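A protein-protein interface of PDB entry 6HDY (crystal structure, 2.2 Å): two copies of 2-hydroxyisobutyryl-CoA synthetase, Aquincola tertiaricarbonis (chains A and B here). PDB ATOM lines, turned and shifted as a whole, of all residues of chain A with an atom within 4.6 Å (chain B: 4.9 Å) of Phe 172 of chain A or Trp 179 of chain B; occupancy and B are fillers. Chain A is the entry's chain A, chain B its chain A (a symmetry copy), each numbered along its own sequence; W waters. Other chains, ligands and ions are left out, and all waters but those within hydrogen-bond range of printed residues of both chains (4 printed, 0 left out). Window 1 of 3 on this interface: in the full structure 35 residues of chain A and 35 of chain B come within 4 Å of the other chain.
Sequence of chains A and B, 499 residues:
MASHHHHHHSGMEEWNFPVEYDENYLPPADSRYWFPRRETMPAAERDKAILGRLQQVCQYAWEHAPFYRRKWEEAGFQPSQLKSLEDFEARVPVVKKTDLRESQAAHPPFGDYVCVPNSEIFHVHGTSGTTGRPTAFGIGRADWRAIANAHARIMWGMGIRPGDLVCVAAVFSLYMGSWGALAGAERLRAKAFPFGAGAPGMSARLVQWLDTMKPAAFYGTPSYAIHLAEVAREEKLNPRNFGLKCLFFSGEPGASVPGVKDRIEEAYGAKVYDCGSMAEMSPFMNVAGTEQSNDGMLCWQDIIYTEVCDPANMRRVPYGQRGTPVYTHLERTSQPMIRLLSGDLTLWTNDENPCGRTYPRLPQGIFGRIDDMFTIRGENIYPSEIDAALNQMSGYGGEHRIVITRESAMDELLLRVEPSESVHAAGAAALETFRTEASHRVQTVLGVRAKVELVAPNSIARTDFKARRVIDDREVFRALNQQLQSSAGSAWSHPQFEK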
ATOM      1  N   VAL A 168      26.730 -17.160  21.902  1.00  0.00           N
ATOM      2  CA  VAL A 168      26.936 -18.620  21.797  1.00  0.00           C
ATOM      3  C   VAL A 168      28.274 -18.823  21.095  1.00  0.00           C
ATOM      4  O   VAL A 168      28.389 -18.659  19.882  1.00  0.00           O
ATOM      5  CB  VAL A 168      25.744 -19.379  21.133  1.00  0.00           C
ATOM      6  CG1 VAL A 168      25.988 -20.887  21.132  1.00  0.00           C
ATOM      7  CG2 VAL A 168      24.449 -19.069  21.877  1.00  0.00           C
ATOM      8  N   ALA A 170      30.557 -21.607  20.867  1.00  0.00           N
ATOM      9  CA  ALA A 170      30.969 -23.007  20.709  1.00  0.00           C
ATOM     10  C   ALA A 170      30.760 -23.290  19.222  1.00  0.00           C
ATOM     11  O   ALA A 170      29.977 -22.581  18.579  1.00  0.00           O
ATOM     12  CB  ALA A 170      30.126 -23.931  21.580  1.00  0.00           C
ATOM     13  N   VAL A 171      31.512 -24.245  18.659  1.00  0.00           N
ATOM     14  CA  VAL A 171      31.493 -24.594  17.242  1.00  0.00           C
ATOM     15  C   VAL A 171      30.082 -25.027  16.786  1.00  0.00           C
ATOM     16  O   VAL A 171      29.415 -25.804  17.460  1.00  0.00           O
ATOM     17  CB  VAL A 171      32.620 -25.619  16.853  1.00  0.00           C
ATOM     18  CG1 VAL A 171      32.487 -26.937  17.616  1.00  0.00           C
ATOM     19  CG2 VAL A 171      32.661 -25.879  15.344  1.00  0.00           C
ATOM     20  N   PHE A 172      29.624 -24.477  15.658  1.00  0.00           N
ATOM     21  CA  PHE A 172      28.321 -24.809  15.088  1.00  0.00           C
ATOM     22  C   PHE A 172      28.563 -25.777  13.961  1.00  0.00           C
ATOM     23  O   PHE A 172      28.979 -25.392  12.864  1.00  0.00           O
ATOM     24  CB  PHE A 172      27.590 -23.552  14.609  1.00  0.00           C
ATOM     25  CG  PHE A 172      26.921 -22.775  15.708  1.00  0.00           C
ATOM     26  CD1 PHE A 172      25.626 -23.072  16.097  1.00  0.00           C
ATOM     27  CD2 PHE A 172      27.577 -21.712  16.329  1.00  0.00           C
ATOM     28  CE1 PHE A 172      25.004 -22.348  17.107  1.00  0.00           C
ATOM     29  CE2 PHE A 172      26.971 -21.010  17.372  1.00  0.00           C
ATOM     30  CZ  PHE A 172      25.682 -21.319  17.739  1.00  0.00           C
ATOM     31  N   SER A 173      28.474 -27.055  14.293  1.00  0.00           N
ATOM     32  CA  SER A 173      28.758 -28.131  13.346  1.00  0.00           C
ATOM     33  C   SER A 173      27.945 -29.355  13.781  1.00  0.00           C
ATOM     34  O   SER A 173      26.781 -29.215  14.132  1.00  0.00           O
ATOM     35  CB  SER A 173      30.262 -28.433  13.343  1.00  0.00           C
ATOM     36  OG  SER A 173      30.593 -29.421  12.374  1.00  0.00           O
ATOM     37  N   SER A 178      26.407 -26.069  20.975  1.00  0.00           N
ATOM     38  CA  SER A 178      26.149 -24.741  20.401  1.00  0.00           C
ATOM     39  C   SER A 178      24.699 -24.569  19.936  1.00  0.00           C
ATOM     40  O   SER A 178      24.069 -23.553  20.253  1.00  0.00           O
ATOM     41  CB  SER A 178      27.088 -24.497  19.231  1.00  0.00           C
ATOM     42  OG  SER A 178      26.948 -25.542  18.284  1.00  0.00           O
ATOM     43  N   TRP A 179      24.171 -25.569  19.178  1.00  0.00           N
ATOM     44  CA  TRP A 179      22.796 -25.543  18.628  1.00  0.00           C
ATOM     45  C   TRP A 179      21.771 -25.517  19.734  1.00  0.00           C
ATOM     46  O   TRP A 179      20.777 -24.799  19.647  1.00  0.00           O
ATOM     47  CB  TRP A 179      22.557 -26.742  17.668  1.00  0.00           C
ATOM     48  CG  TRP A 179      23.487 -26.727  16.491  1.00  0.00           C
ATOM     49  CD1 TRP A 179      24.640 -27.438  16.354  1.00  0.00           C
ATOM     50  CD2 TRP A 179      23.385 -25.893  15.322  1.00  0.00           C
ATOM     51  NE1 TRP A 179      25.255 -27.121  15.167  1.00  0.00           N
ATOM     52  CE2 TRP A 179      24.512 -26.168  14.514  1.00  0.00           C
ATOM     53  CE3 TRP A 179      22.465 -24.920  14.892  1.00  0.00           C
ATOM     54  CZ2 TRP A 179      24.738 -25.522  13.285  1.00  0.00           C
ATOM     55  CZ3 TRP A 179      22.695 -24.267  13.682  1.00  0.00           C
ATOM     56  CH2 TRP A 179      23.811 -24.578  12.887  1.00  0.00           C
ATOM     57  N   LEU A 182      21.773 -22.031  21.352  1.00  0.00           N
ATOM     58  CA  LEU A 182      21.169 -21.117  20.391  1.00  0.00           C
ATOM     59  C   LEU A 182      19.617 -21.247  20.373  1.00  0.00           C
ATOM     60  O   LEU A 182      18.918 -20.226  20.383  1.00  0.00           O
ATOM     61  CB  LEU A 182      21.757 -21.366  18.991  1.00  0.00           C
ATOM     62  CG  LEU A 182      21.045 -20.711  17.810  1.00  0.00           C
ATOM     63  CD1 LEU A 182      21.154 -19.190  17.874  1.00  0.00           C
ATOM     64  CD2 LEU A 182      21.562 -21.245  16.515  1.00  0.00           C
ATOM     65  N   PRO A 194      25.060 -15.961  17.715  1.00  0.00           N
ATOM     66  CA  PRO A 194      25.833 -17.187  17.452  1.00  0.00           C
ATOM     67  C   PRO A 194      27.176 -16.931  16.769  1.00  0.00           C
ATOM     68  O   PRO A 194      27.344 -17.156  15.569  1.00  0.00           O
ATOM     69  CB  PRO A 194      24.861 -18.029  16.627  1.00  0.00           C
ATOM     70  CG  PRO A 194      24.054 -17.031  15.861  1.00  0.00           C
ATOM     71  CD  PRO A 194      24.012 -15.767  16.683  1.00  0.00           C
ATOM     72  N   GLY A 196      29.986 -18.561  17.489  1.00  0.00           N
ATOM     73  CA  GLY A 196      30.627 -19.837  17.193  1.00  0.00           C
ATOM     74  C   GLY A 196      32.061 -19.908  17.645  1.00  0.00           C
ATOM     75  O   GLY A 196      32.499 -19.090  18.451  1.00  0.00           O
ATOM     76  N   HIS B 123      18.438 -12.255  16.003  1.00  0.00           N
ATOM     77  CA  HIS B 123      19.792 -12.743  15.747  1.00  0.00           C
ATOM     78  C   HIS B 123      20.750 -11.608  15.524  1.00  0.00           C
ATOM     79  O   HIS B 123      20.377 -10.587  14.937  1.00  0.00           O
ATOM     80  CB  HIS B 123      19.795 -13.608  14.506  1.00  0.00           C
ATOM     81  CG  HIS B 123      19.771 -15.080  14.744  1.00  0.00           C
ATOM     82  ND1 HIS B 123      20.572 -15.925  14.022  1.00  0.00           N
ATOM     83  CD2 HIS B 123      18.984 -15.815  15.556  1.00  0.00           C
ATOM     84  CE1 HIS B 123      20.228 -17.145  14.383  1.00  0.00           C
ATOM     85  NE2 HIS B 123      19.291 -17.123  15.319  1.00  0.00           N
ATOM     86  N   HIS B 125      24.491 -10.919  13.880  1.00  0.00           N
ATOM     87  CA  HIS B 125      25.525 -11.381  12.958  1.00  0.00           C
ATOM     88  C   HIS B 125      26.309 -10.170  12.529  1.00  0.00           C
ATOM     89  O   HIS B 125      26.174  -9.121  13.129  1.00  0.00           O
ATOM     90  CB  HIS B 125      24.892 -12.092  11.754  1.00  0.00           C
ATOM     91  CG  HIS B 125      24.187 -13.357  12.112  1.00  0.00           C
ATOM     92  ND1 HIS B 125      24.877 -14.546  12.272  1.00  0.00           N
ATOM     93  CD2 HIS B 125      22.868 -13.574  12.338  1.00  0.00           C
ATOM     94  CE1 HIS B 125      23.964 -15.437  12.617  1.00  0.00           C
ATOM     95  NE2 HIS B 125      22.737 -14.905  12.641  1.00  0.00           N
ATOM     96  N   TRP B 144      13.751 -12.787   9.961  1.00  0.00           N
ATOM     97  CA  TRP B 144      14.355 -14.126   9.922  1.00  0.00           C
ATOM     98  C   TRP B 144      13.371 -15.086   9.207  1.00  0.00           C
ATOM     99  O   TRP B 144      13.773 -15.864   8.333  1.00  0.00           O
ATOM    100  CB  TRP B 144      14.718 -14.614  11.369  1.00  0.00           C
ATOM    101  CG  TRP B 144      15.718 -15.733  11.334  1.00  0.00           C
ATOM    102  CD1 TRP B 144      15.444 -17.062  11.201  1.00  0.00           C
ATOM    103  CD2 TRP B 144      17.145 -15.599  11.183  1.00  0.00           C
ATOM    104  NE1 TRP B 144      16.615 -17.776  11.050  1.00  0.00           N
ATOM    105  CE2 TRP B 144      17.677 -16.903  11.054  1.00  0.00           C
ATOM    106  CE3 TRP B 144      18.028 -14.503  11.151  1.00  0.00           C
ATOM    107  CZ2 TRP B 144      19.059 -17.144  10.903  1.00  0.00           C
ATOM    108  CZ3 TRP B 144      19.402 -14.744  11.042  1.00  0.00           C
ATOM    109  CH2 TRP B 144      19.901 -16.050  10.916  1.00  0.00           C
ATOM    110  N   PHE B 172      29.521 -21.122  10.408  1.00  0.00           N
ATOM    111  CA  PHE B 172      28.355 -20.624  11.133  1.00  0.00           C
ATOM    112  C   PHE B 172      28.862 -19.706  12.213  1.00  0.00           C
ATOM    113  O   PHE B 172      29.355 -20.152  13.253  1.00  0.00           O
ATOM    114  CB  PHE B 172      27.528 -21.776  11.710  1.00  0.00           C
ATOM    115  CG  PHE B 172      26.630 -22.449  10.708  1.00  0.00           C
ATOM    116  CD1 PHE B 172      25.348 -21.978  10.480  1.00  0.00           C
ATOM    117  CD2 PHE B 172      27.057 -23.584  10.019  1.00  0.00           C
ATOM    118  CE1 PHE B 172      24.515 -22.605   9.561  1.00  0.00           C
ATOM    119  CE2 PHE B 172      26.238 -24.191   9.065  1.00  0.00           C
ATOM    120  CZ  PHE B 172      24.966 -23.709   8.859  1.00  0.00           C
ATOM    121  N   SER B 173      28.903 -18.425  11.884  1.00  0.00           N
ATOM    122  CA  SER B 173      29.443 -17.404  12.779  1.00  0.00           C
ATOM    123  C   SER B 173      28.753 -16.079  12.438  1.00  0.00           C
ATOM    124  O   SER B 173      27.546 -16.060  12.236  1.00  0.00           O
ATOM    125  CB  SER B 173      30.963 -17.306  12.594  1.00  0.00           C
ATOM    126  OG  SER B 173      31.540 -16.379  13.505  1.00  0.00           O
ATOM    127  N   TYR B 175      29.089 -14.516   9.641  1.00  0.00           N
ATOM    128  CA  TYR B 175      28.772 -14.705   8.224  1.00  0.00           C
ATOM    129  C   TYR B 175      27.321 -15.159   7.943  1.00  0.00           C
ATOM    130  O   TYR B 175      26.892 -16.216   8.414  1.00  0.00           O
ATOM    131  CB  TYR B 175      29.803 -15.670   7.631  1.00  0.00           C
ATOM    132  CG  TYR B 175      29.645 -15.892   6.145  1.00  0.00           C
ATOM    133  CD1 TYR B 175      29.781 -14.839   5.247  1.00  0.00           C
ATOM    134  CD2 TYR B 175      29.380 -17.160   5.633  1.00  0.00           C
ATOM    135  CE1 TYR B 175      29.665 -15.041   3.871  1.00  0.00           C
ATOM    136  CE2 TYR B 175      29.275 -17.377   4.256  1.00  0.00           C
ATOM    137  CZ  TYR B 175      29.409 -16.310   3.381  1.00  0.00           C
ATOM    138  OH  TYR B 175      29.306 -16.490   2.029  1.00  0.00           O
ATOM    139  N   MET B 176      26.587 -14.381   7.107  1.00  0.00           N
ATOM    140  CA  MET B 176      25.169 -14.636   6.808  1.00  0.00           C
ATOM    141  C   MET B 176      24.867 -15.805   5.882  1.00  0.00           C
ATOM    142  O   MET B 176      23.751 -16.336   5.939  1.00  0.00           O
ATOM    143  CB  MET B 176      24.473 -13.387   6.261  1.00  0.00           C
ATOM    144  CG  MET B 176      24.261 -12.294   7.306  1.00  0.00           C
ATOM    145  SD  MET B 176      23.201 -12.755   8.680  1.00  0.00           S
ATOM    146  CE  MET B 176      21.615 -13.000   7.890  1.00  0.00           C
ATOM    147  N   GLY B 177      25.822 -16.142   5.007  1.00  0.00           N
ATOM    148  CA  GLY B 177      25.696 -17.184   4.012  1.00  0.00           C
ATOM    149  C   GLY B 177      25.185 -18.500   4.541  1.00  0.00           C
ATOM    150  O   GLY B 177      24.180 -19.022   4.047  1.00  0.00           O
ATOM    151  N   SER B 178      25.910 -19.071   5.519  1.00  0.00           N
ATOM    152  CA  SER B 178      25.551 -20.358   6.131  1.00  0.00           C
ATOM    153  C   SER B 178      24.160 -20.339   6.774  1.00  0.00           C
ATOM    154  O   SER B 178      23.366 -21.259   6.546  1.00  0.00           O
ATOM    155  CB  SER B 178      26.587 -20.735   7.177  1.00  0.00           C
ATOM    156  OG  SER B 178      26.706 -19.688   8.126  1.00  0.00           O
ATOM    157  N   TRP B 179      23.868 -19.284   7.583  1.00  0.00           N
ATOM    158  CA  TRP B 179      22.580 -19.131   8.299  1.00  0.00           C
ATOM    159  C   TRP B 179      21.432 -19.011   7.329  1.00  0.00           C
ATOM    160  O   TRP B 179      20.370 -19.591   7.545  1.00  0.00           O
ATOM    161  CB  TRP B 179      22.625 -17.919   9.271  1.00  0.00           C
ATOM    162  CG  TRP B 179      23.683 -18.068  10.324  1.00  0.00           C
ATOM    163  CD1 TRP B 179      24.928 -17.518  10.311  1.00  0.00           C
ATOM    164  CD2 TRP B 179      23.617 -18.890  11.504  1.00  0.00           C
ATOM    165  NE1 TRP B 179      25.638 -17.923  11.415  1.00  0.00           N
ATOM    166  CE2 TRP B 179      24.862 -18.775  12.163  1.00  0.00           C
ATOM    167  CE3 TRP B 179      22.635 -19.735  12.052  1.00  0.00           C
ATOM    168  CZ2 TRP B 179      25.150 -19.455  13.360  1.00  0.00           C
ATOM    169  CZ3 TRP B 179      22.925 -20.423  13.230  1.00  0.00           C
ATOM    170  CH2 TRP B 179      24.163 -20.270  13.878  1.00  0.00           C
ATOM    171  N   GLY B 180      21.651 -18.282   6.249  1.00  0.00           N
ATOM    172  CA  GLY B 180      20.637 -18.111   5.210  1.00  0.00           C
ATOM    173  C   GLY B 180      20.277 -19.387   4.483  1.00  0.00           C
ATOM    174  O   GLY B 180      19.101 -19.630   4.223  1.00  0.00           O
ATOM    175  N   ALA B 181      21.273 -20.230   4.172  1.00  0.00           N
ATOM    176  CA  ALA B 181      21.007 -21.511   3.510  1.00  0.00           C
ATOM    177  C   ALA B 181      20.340 -22.485   4.480  1.00  0.00           C
ATOM    178  O   ALA B 181      19.448 -23.251   4.082  1.00  0.00           O
ATOM    179  CB  ALA B 181      22.291 -22.110   2.948  1.00  0.00           C
ATOM    180  N   LEU B 182      20.769 -22.452   5.753  1.00  0.00           N
ATOM    181  CA  LEU B 182      20.172 -23.286   6.789  1.00  0.00           C
ATOM    182  C   LEU B 182      18.666 -22.951   6.998  1.00  0.00           C
ATOM    183  O   LEU B 182      17.841 -23.870   7.083  1.00  0.00           O
ATOM    184  CB  LEU B 182      20.958 -23.129   8.102  1.00  0.00           C
ATOM    185  CG  LEU B 182      20.316 -23.694   9.368  1.00  0.00           C
ATOM    186  CD1 LEU B 182      20.214 -25.215   9.304  1.00  0.00           C
ATOM    187  CD2 LEU B 182      21.057 -23.243  10.584  1.00  0.00           C
ATOM    188  N   ALA B 183      18.329 -21.635   7.104  1.00  0.00           N
ATOM    189  CA  ALA B 183      16.953 -21.159   7.322  1.00  0.00           C
ATOM    190  C   ALA B 183      16.031 -21.583   6.181  1.00  0.00           C
ATOM    191  O   ALA B 183      14.879 -21.911   6.428  1.00  0.00           O
ATOM    192  CB  ALA B 183      16.915 -19.646   7.522  1.00  0.00           C
ATOM    193  N   PRO B 194      23.644 -28.937   9.004  1.00  0.00           N
ATOM    194  CA  PRO B 194      24.600 -27.827   9.159  1.00  0.00           C
ATOM    195  C   PRO B 194      25.971 -28.265   9.672  1.00  0.00           C
ATOM    196  O   PRO B 194      26.315 -28.075  10.840  1.00  0.00           O
ATOM    197  CB  PRO B 194      23.858 -26.870  10.091  1.00  0.00           C
ATOM    198  CG  PRO B 194      23.027 -27.758  10.959  1.00  0.00           C
ATOM    199  CD  PRO B 194      22.716 -28.998  10.160  1.00  0.00           C
ATOM    200  N   PHE B 195      26.779 -28.852   8.766  1.00  0.00           N
ATOM    201  CA  PHE B 195      28.124 -29.287   9.145  1.00  0.00           C
ATOM    202  C   PHE B 195      29.024 -28.072   9.371  1.00  0.00           C
ATOM    203  O   PHE B 195      29.858 -28.098  10.247  1.00  0.00           O
ATOM    204  CB  PHE B 195      28.728 -30.264   8.099  1.00  0.00           C
ATOM    205  CG  PHE B 195      30.054 -30.859   8.516  1.00  0.00           C
ATOM    206  CD1 PHE B 195      31.252 -30.210   8.221  1.00  0.00           C
ATOM    207  CD2 PHE B 195      30.110 -32.086   9.170  1.00  0.00           C
ATOM    208  CE1 PHE B 195      32.486 -30.761   8.602  1.00  0.00           C
ATOM    209  CE2 PHE B 195      31.342 -32.623   9.580  1.00  0.00           C
ATOM    210  CZ  PHE B 195      32.524 -31.957   9.289  1.00  0.00           C
ATOM    211  N   GLY B 196      28.862 -27.018   8.595  1.00  0.00           N
ATOM    212  CA  GLY B 196      29.699 -25.841   8.799  1.00  0.00           C
ATOM    213  C   GLY B 196      31.062 -25.958   8.172  1.00  0.00           C
ATOM    214  O   GLY B 196      31.284 -26.820   7.325  1.00  0.00           O
HETATM  215  O   HOH W   1      30.944 -22.117  14.523  1.00  0.00           O
HETATM  216  O   HOH W   2      30.646 -23.646  11.391  1.00  0.00           O
HETATM  217  O   HOH W   3      25.672 -31.099  11.685  1.00  0.00           O
HETATM  218  O   HOH W   4      27.010 -14.066  14.786  1.00  0.00           O
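Val 168 of chain A touches none of the printed residues of chain B.
Of the printed residues of chain B, Phe 172 of chain A touches Phe 172 (3.4 Å), Trp 179 (3.9 Å) and Phe 195 (3.9 Å).
Of the printed residues of chain B, Ser 173 of chain A touches Pro 194 (3.5 Å) and Phe 195 (2.6 Å).
Of the printed residues of chain B, Pro 194 of chain A touches His 125, Ser 173 and Trp 179.
Of the printed residues of chain A, His 125 of chain B touches Pro 194.
Of chain A, only Phe 172, Trp 179, Leu 182 and Pro 194 come within 4 Å of Trp 179 of chain B.
Of the printed residues of chain A, Pro 194 of chain B touches Ser 173 (3.5 Å) and Trp 179 (3.6 Å).
The nearest printed residue of chain A that does not touch Phe 195 of chain B is Trp 179 of chain A (6.0 Å).
A ring nitrogen (ND1) of His 123 of chain B is in hydrogen-bond range of a ring nitrogen (NE2) of His 125 of chain B (2.8 Å).
The indole nitrogen (NE1) of Trp 179 of chain A is in hydrogen-bond range of the backbone carbonyl oxygen (O) of Ser 173 of chain A (2.8 Å).
ND1 of His 125 of chain B is in hydrogen-bond range of O of Ser 173 of chain B (3.1 Å).
The backbone carbonyl oxygen of Ser 173 of chain B lies within hydrogen-bond range of the indole nitrogen of Trp 179 of chain B (2.8 Å).
The side-chain hydroxyl of Ser 173 of chain A lies within hydrogen-bond range of the backbone carbonyl oxygen of Phe 195 of chain B, at 2.6 Å.
Phe 172 of chain A touches Trp 179 of chain B (CD1 to CH2, 3.9 Å).
Phe 195 of chain B touches Phe 172 of chain A (O to O, 3.9 Å).
CA of Ser 173 of chain A touches O of Pro 194 of chain B, 3.5 Å away.
Phe 172 of chain B touches Trp 179 of chain A.
Trp 179 of chain A touches Trp 179 of chain B (CZ3 to CZ3, 3.9 Å).
Trp 179 of chain A touches Leu 182 of chain B (CZ3 to CD2, 3.7 Å).
Trp 179 of chain A touches Pro 194 of chain B (CZ2 to CB, 3.6 Å).
Leu 182 of chain A touches His 123 of chain B.
His 125 of chain B touches Pro 194 of chain A (CE1 to CG, 3.6 Å).
Pro 194 of chain A touches Ser 173 of chain B (O to CA, 3.5 Å).
Printed residues of chain B that touch a printed residue of chain A: His 123, His 125, Phe 172, Ser 173, Trp 179, Leu 182, Pro 194 and Phe 195.
Hydrophobic or aromatic side chains of chain B within 4 Å of the printed part of chain A: His 123, His 125, Phe 172, Trp 179, Leu 182 and Pro 194.
Of the 10 printed residues of chain A, 5 touch a printed residue of chain B.
Hydrophobic or aromatic side chains of chain A within 4 Å of the printed part of chain B: Phe 172, Trp 179, Leu 182 and Pro 194.
Among the printed residues, 14 pairs touch across the chains.
Water W2 bridges the backbone carbonyl oxygen (O) of Phe 172 of chain A (2.8 Å) and the backbone NH (N) of Phe 172 of chain B (2.9 Å).
Water W1 bridges the backbone carbonyl oxygen (O) of Phe 172 of chain B (2.8 Å) and the backbone NH (N) of Phe 172 of chain A (2.9 Å).
Water W3 bridges the backbone carbonyl oxygen of Pro 194 of chain B (3.2 Å) and the backbone carbonyl oxygen of Ser 173 of chain A (3.3 Å).
Water W4 lies within hydrogen-bond range of the backbone carbonyl oxygen of Pro 194 of chain A (3.2 Å), the backbone carbonyl oxygen of Ser 173 of chain B (3.3 Å) and a ring nitrogen (ND1) of His 125 of chain B (3.3 Å).
Phe 172 of chain A touches its own counterpart, Phe 172 of chain B.
Ser 173 of chain A touches Pro 194 of chain B, and with the chains exchanged Pro 194 of chain A touches Ser 173 of chain B.
Trp 179 of chain A touches Leu 182 of chain B, and with the chains exchanged Leu 182 of chain A touches Trp 179 of chain B.
Trp 179 of chain A touches Pro 194 of chain B, and with the chains exchanged Pro 194 of chain A touches Trp 179 of chain B.
Positions printed for both chains: 172, 173, 178, 179, 182, 194 and 196.
Of the 14 pairs that touch across the chains among the printed residues, 10 have their exchanged pair printed and touching as well.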
